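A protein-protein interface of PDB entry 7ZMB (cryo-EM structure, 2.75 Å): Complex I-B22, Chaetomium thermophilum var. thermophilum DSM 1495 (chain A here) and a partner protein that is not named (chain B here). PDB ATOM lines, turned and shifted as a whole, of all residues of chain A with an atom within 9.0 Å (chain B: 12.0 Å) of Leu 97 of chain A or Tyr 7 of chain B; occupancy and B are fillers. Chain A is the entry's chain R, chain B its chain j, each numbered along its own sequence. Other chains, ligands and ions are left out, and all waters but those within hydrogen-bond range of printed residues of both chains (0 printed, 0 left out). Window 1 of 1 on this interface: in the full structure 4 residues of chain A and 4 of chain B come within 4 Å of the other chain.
Of the 8 printed residues of chain A, 4 touch a printed residue of chain B. Along chain B the printed residues that touch a printed residue of chain A span positions 4 to 7. Among the printed residues, 8 pairs touch across the chains.
Pro 94 of chain A touches just one residue of chain B: Tyr 7. Pro 95 of chain A touches just one residue of chain B: Tyr 7. Pro 96 of chain A touches none of the printed residues of chain B. Of chain B, only His 6 (3.8 Å) and Tyr 7 (3.6 Å) come within 4 Å of Leu 97 of chain A. No residue of chain B comes within 4 Å of Lys 98 of chain A. Of chain B, only Leu 4, Gln 5, His 6 and Tyr 7 come within 4 Å of Phe 99 of chain A. Gly 3 of chain B touches none of the printed residues of chain A. Printed residues of chain A within 4 Å of Leu 4 of chain B: Phe 99. Of the printed residues of chain A, Gln 5 of chain B touches Phe 99. Tyr 7 of chain B touches four residues of chain A. Lys 8 of chain B touches none of the printed residues of chain A. The nearest residue of chain A that does not touch Tyr 7 of chain B is Pro 96 of chain A (6.1 Å). The nearest printed residue of chain A that does not touch Leu 4 of chain B is Lys 98 of chain A (4.8 Å).
Tyr 7 of chain B touches Pro 94 of chain A (OH to CB, 3.9 Å). Pro 95 of chain A touches Tyr 7 of chain B (CD to CE1, 3.6 Å). CD1 of Leu 97 of chain A touches O of His 6 of chain B, at 3.8 Å. CD1 of Leu 97 of chain A touches CE1 of Tyr 7 of chain B (3.6 Å). CD1 of Leu 4 of chain B touches CE1 of Phe 99 of chain A, 3.7 Å away. Phe 99 of chain A touches Gln 5 of chain B (CE1 to O, 3.7 Å). CZ of Phe 99 of chain A touches CA of His 6 of chain B, 3.7 Å away. Tyr 7 of chain B touches Phe 99 of chain A (CE2 to CE2, 3.3 Å).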
ATOM      1  N   ASN A  90      18.747 -19.873   0.435  1.00  0.00           N
ATOM      2  CA  ASN A  90      17.503 -19.133   0.263  1.00  0.00           C
ATOM      3  C   ASN A  90      16.412 -19.838   1.054  1.00  0.00           C
ATOM      4  O   ASN A  90      15.916 -20.890   0.635  1.00  0.00           O
ATOM      5  CB  ASN A  90      17.150 -19.036  -1.222  1.00  0.00           C
ATOM      6  CG  ASN A  90      15.907 -18.232  -1.479  1.00  0.00           C
ATOM      7  OD1 ASN A  90      15.379 -17.585  -0.589  1.00  0.00           O
ATOM      8  ND2 ASN A  90      15.439 -18.257  -2.716  1.00  0.00           N
ATOM      9  N   PRO A  93      10.076 -19.309   0.727  1.00  0.00           N
ATOM     10  CA  PRO A  93       9.419 -20.290  -0.136  1.00  0.00           C
ATOM     11  C   PRO A  93       9.313 -19.782  -1.562  1.00  0.00           C
ATOM     12  O   PRO A  93       9.325 -18.564  -1.807  1.00  0.00           O
ATOM     13  CB  PRO A  93       8.027 -20.450   0.504  1.00  0.00           C
ATOM     14  CG  PRO A  93       8.115 -19.783   1.851  1.00  0.00           C
ATOM     15  CD  PRO A  93       9.155 -18.730   1.718  1.00  0.00           C
ATOM     16  N   PRO A  94       9.216 -20.684  -2.543  1.00  0.00           N
ATOM     17  CA  PRO A  94       9.129 -20.246  -3.932  1.00  0.00           C
ATOM     18  C   PRO A  94       7.825 -19.520  -4.203  1.00  0.00           C
ATOM     19  O   PRO A  94       6.784 -19.833  -3.599  1.00  0.00           O
ATOM     20  CB  PRO A  94       9.212 -21.566  -4.722  1.00  0.00           C
ATOM     21  CG  PRO A  94       9.875 -22.511  -3.787  1.00  0.00           C
ATOM     22  CD  PRO A  94       9.351 -22.144  -2.441  1.00  0.00           C
ATOM     23  N   PRO A  95       7.823 -18.565  -5.127  1.00  0.00           N
ATOM     24  CA  PRO A  95       6.636 -17.743  -5.362  1.00  0.00           C
ATOM     25  C   PRO A  95       5.596 -18.499  -6.167  1.00  0.00           C
ATOM     26  O   PRO A  95       5.891 -19.561  -6.736  1.00  0.00           O
ATOM     27  CB  PRO A  95       7.200 -16.560  -6.159  1.00  0.00           C
ATOM     28  CG  PRO A  95       8.289 -17.172  -6.938  1.00  0.00           C
ATOM     29  CD  PRO A  95       8.921 -18.197  -6.034  1.00  0.00           C
ATOM     30  N   PRO A  96       4.371 -17.983  -6.254  1.00  0.00           N
ATOM     31  CA  PRO A  96       3.339 -18.692  -7.018  1.00  0.00           C
ATOM     32  C   PRO A  96       3.586 -18.658  -8.516  1.00  0.00           C
ATOM     33  O   PRO A  96       3.407 -17.623  -9.166  1.00  0.00           O
ATOM     34  CB  PRO A  96       2.054 -17.942  -6.647  1.00  0.00           C
ATOM     35  CG  PRO A  96       2.512 -16.584  -6.256  1.00  0.00           C
ATOM     36  CD  PRO A  96       3.836 -16.784  -5.586  1.00  0.00           C
ATOM     37  N   LEU A  97       4.003 -19.791  -9.072  1.00  0.00           N
ATOM     38  CA  LEU A  97       4.179 -19.947 -10.507  1.00  0.00           C
ATOM     39  C   LEU A  97       3.535 -21.247 -10.953  1.00  0.00           C
ATOM     40  O   LEU A  97       3.513 -22.233 -10.212  1.00  0.00           O
ATOM     41  CB  LEU A  97       5.657 -19.938 -10.905  1.00  0.00           C
ATOM     42  CG  LEU A  97       6.295 -18.567 -11.117  1.00  0.00           C
ATOM     43  CD1 LEU A  97       7.664 -18.709 -11.736  1.00  0.00           C
ATOM     44  CD2 LEU A  97       5.408 -17.701 -11.985  1.00  0.00           C
ATOM     45  N   LYS A  98       3.007 -21.241 -12.170  1.00  0.00           N
ATOM     46  CA  LYS A  98       2.379 -22.422 -12.757  1.00  0.00           C
ATOM     47  C   LYS A  98       3.415 -23.121 -13.629  1.00  0.00           C
ATOM     48  O   LYS A  98       3.721 -22.670 -14.736  1.00  0.00           O
ATOM     49  CB  LYS A  98       1.135 -22.040 -13.554  1.00  0.00           C
ATOM     50  CG  LYS A  98      -0.123 -21.867 -12.716  1.00  0.00           C
ATOM     51  CD  LYS A  98      -0.095 -20.583 -11.900  1.00  0.00           C
ATOM     52  CE  LYS A  98      -0.212 -19.362 -12.795  1.00  0.00           C
ATOM     53  NZ  LYS A  98      -0.250 -18.101 -12.005  1.00  0.00           N
ATOM     54  N   PHE A  99       3.955 -24.226 -13.125  1.00  0.00           N
ATOM     55  CA  PHE A  99       4.942 -25.007 -13.860  1.00  0.00           C
ATOM     56  C   PHE A  99       4.432 -26.419 -14.124  1.00  0.00           C
ATOM     57  O   PHE A  99       4.918 -27.106 -15.022  1.00  0.00           O
ATOM     58  CB  PHE A  99       6.265 -25.059 -13.094  1.00  0.00           C
ATOM     59  CG  PHE A  99       7.123 -23.854 -13.302  1.00  0.00           C
ATOM     60  CD1 PHE A  99       7.348 -23.365 -14.571  1.00  0.00           C
ATOM     61  CD2 PHE A  99       7.689 -23.194 -12.230  1.00  0.00           C
ATOM     62  CE1 PHE A  99       8.130 -22.254 -14.766  1.00  0.00           C
ATOM     63  CE2 PHE A  99       8.466 -22.080 -12.425  1.00  0.00           C
ATOM     64  CZ  PHE A  99       8.688 -21.610 -13.688  1.00  0.00           C
ATOM     65  N   GLY B   3       7.041 -19.747 -23.851  1.00  0.00           N
ATOM     66  CA  GLY B   3       6.256 -18.529 -23.780  1.00  0.00           C
ATOM     67  C   GLY B   3       5.954 -18.098 -22.359  1.00  0.00           C
ATOM     68  O   GLY B   3       5.748 -16.915 -22.090  1.00  0.00           O
ATOM     69  N   LEU B   4       5.926 -19.066 -21.448  1.00  0.00           N
ATOM     70  CA  LEU B   4       5.668 -18.774 -20.048  1.00  0.00           C
ATOM     71  C   LEU B   4       6.898 -18.142 -19.401  1.00  0.00           C
ATOM     72  O   LEU B   4       8.010 -18.181 -19.933  1.00  0.00           O
ATOM     73  CB  LEU B   4       5.252 -20.047 -19.309  1.00  0.00           C
ATOM     74  CG  LEU B   4       6.213 -21.241 -19.287  1.00  0.00           C
ATOM     75  CD1 LEU B   4       7.226 -21.156 -18.151  1.00  0.00           C
ATOM     76  CD2 LEU B   4       5.435 -22.549 -19.221  1.00  0.00           C
ATOM     77  N   GLN B   5       6.685 -17.549 -18.231  1.00  0.00           N
ATOM     78  CA  GLN B   5       7.760 -16.937 -17.466  1.00  0.00           C
ATOM     79  C   GLN B   5       8.292 -17.921 -16.435  1.00  0.00           C
ATOM     80  O   GLN B   5       7.557 -18.761 -15.911  1.00  0.00           O
ATOM     81  CB  GLN B   5       7.291 -15.648 -16.784  1.00  0.00           C
ATOM     82  CG  GLN B   5       6.267 -15.848 -15.685  1.00  0.00           C
ATOM     83  CD  GLN B   5       6.042 -14.588 -14.876  1.00  0.00           C
ATOM     84  OE1 GLN B   5       6.973 -14.045 -14.281  1.00  0.00           O
ATOM     85  NE2 GLN B   5       4.802 -14.115 -14.848  1.00  0.00           N
ATOM     86  N   HIS B   6       9.590 -17.809 -16.158  1.00  0.00           N
ATOM     87  CA  HIS B   6      10.328 -18.719 -15.300  1.00  0.00           C
ATOM     88  C   HIS B   6      10.727 -18.008 -14.011  1.00  0.00           C
ATOM     89  O   HIS B   6      10.322 -16.874 -13.751  1.00  0.00           O
ATOM     90  CB  HIS B   6      11.551 -19.261 -16.040  1.00  0.00           C
ATOM     91  CG  HIS B   6      12.419 -18.198 -16.633  1.00  0.00           C
ATOM     92  ND1 HIS B   6      13.571 -17.755 -16.026  1.00  0.00           N
ATOM     93  CD2 HIS B   6      12.300 -17.487 -17.777  1.00  0.00           C
ATOM     94  CE1 HIS B   6      14.126 -16.819 -16.771  1.00  0.00           C
ATOM     95  NE2 HIS B   6      13.374 -16.635 -17.839  1.00  0.00           N
ATOM     96  N   TYR B   7      11.525 -18.690 -13.193  1.00  0.00           N
ATOM     97  CA  TYR B   7      12.013 -18.097 -11.960  1.00  0.00           C
ATOM     98  C   TYR B   7      13.089 -17.062 -12.252  1.00  0.00           C
ATOM     99  O   TYR B   7      13.639 -16.986 -13.352  1.00  0.00           O
ATOM    100  CB  TYR B   7      12.566 -19.164 -11.017  1.00  0.00           C
ATOM    101  CG  TYR B   7      11.500 -19.987 -10.347  1.00  0.00           C
ATOM    102  CD1 TYR B   7      10.510 -19.382  -9.600  1.00  0.00           C
ATOM    103  CD2 TYR B   7      11.477 -21.366 -10.474  1.00  0.00           C
ATOM    104  CE1 TYR B   7       9.526 -20.118  -8.994  1.00  0.00           C
ATOM    105  CE2 TYR B   7      10.502 -22.119  -9.862  1.00  0.00           C
ATOM    106  CZ  TYR B   7       9.522 -21.487  -9.126  1.00  0.00           C
ATOM    107  OH  TYR B   7       8.534 -22.221  -8.515  1.00  0.00           O
ATOM    108  N   LYS B   8      13.379 -16.249 -11.242  1.00  0.00           N
ATOM    109  CA  LYS B   8      14.329 -15.158 -11.388  1.00  0.00           C
ATOM    110  C   LYS B   8      15.748 -15.658 -11.146  1.00  0.00           C
ATOM    111  O   LYS B   8      16.024 -16.303 -10.128  1.00  0.00           O
ATOM    112  CB  LYS B   8      13.985 -14.024 -10.426  1.00  0.00           C
ATOM    113  CG  LYS B   8      12.857 -13.101 -10.880  1.00  0.00           C
ATOM    114  CD  LYS B   8      11.489 -13.758 -10.781  1.00  0.00           C
ATOM    115  CE  LYS B   8      10.386 -12.778 -11.149  1.00  0.00           C
ATOM    116  NZ  LYS B   8       9.045 -13.422 -11.174  1.00  0.00           N
ATOM    117  N   ILE B   9      16.647 -15.350 -12.079  1.00  0.00           N
ATOM    118  CA  ILE B   9      17.978 -15.942 -12.131  1.00  0.00           C
ATOM    119  C   ILE B   9      19.018 -14.830 -12.203  1.00  0.00           C
ATOM    120  O   ILE B   9      18.857 -13.861 -12.950  1.00  0.00           O
ATOM    121  CB  ILE B   9      18.110 -16.893 -13.341  1.00  0.00           C
ATOM    122  CG1 ILE B   9      17.104 -18.045 -13.233  1.00  0.00           C
ATOM    123  CG2 ILE B   9      19.538 -17.413 -13.477  1.00  0.00           C
ATOM    124  CD1 ILE B   9      17.524 -19.160 -12.309  1.00  0.00           C
ATOM    125  N   ALA B  10      20.094 -14.973 -11.426  1.00  0.00           N
ATOM    126  CA  ALA B  10      21.213 -14.031 -11.467  1.00  0.00           C
ATOM    127  C   ALA B  10      22.089 -14.369 -12.669  1.00  0.00           C
ATOM    128  O   ALA B  10      23.163 -14.964 -12.558  1.00  0.00           O
ATOM    129  CB  ALA B  10      22.008 -14.071 -10.172  1.00  0.00           C
ATOM    130  N   MET B  11      21.613 -13.970 -13.843  1.00  0.00           N
ATOM    131  CA  MET B  11      22.324 -14.237 -15.082  1.00  0.00           C
ATOM    132  C   MET B  11      23.664 -13.523 -15.086  1.00  0.00           C
ATOM    133  O   MET B  11      23.728 -12.293 -14.994  1.00  0.00           O
ATOM    134  CB  MET B  11      21.474 -13.791 -16.268  1.00  0.00           C
ATOM    135  CG  MET B  11      20.198 -14.586 -16.435  1.00  0.00           C
ATOM    136  SD  MET B  11      20.502 -16.337 -16.724  1.00  0.00           S
ATOM    137  CE  MET B  11      21.212 -16.282 -18.366  1.00  0.00           C
ATOM    138  N   ASP B  12      24.734 -14.296 -15.204  1.00  0.00           N
ATOM    139  CA  ASP B  12      26.079 -13.755 -15.151  1.00  0.00           C
ATOM    140  C   ASP B  12      26.550 -13.423 -16.557  1.00  0.00           C
ATOM    141  O   ASP B  12      26.734 -14.341 -17.364  1.00  0.00           O
ATOM    142  CB  ASP B  12      27.025 -14.754 -14.517  1.00  0.00           C
ATOM    143  CG  ASP B  12      28.357 -14.145 -14.150  1.00  0.00           C
ATOM    144  OD1 ASP B  12      28.575 -12.951 -14.419  1.00  0.00           O
ATOM    145  OD2 ASP B  12      29.193 -14.871 -13.582  1.00  0.00           O
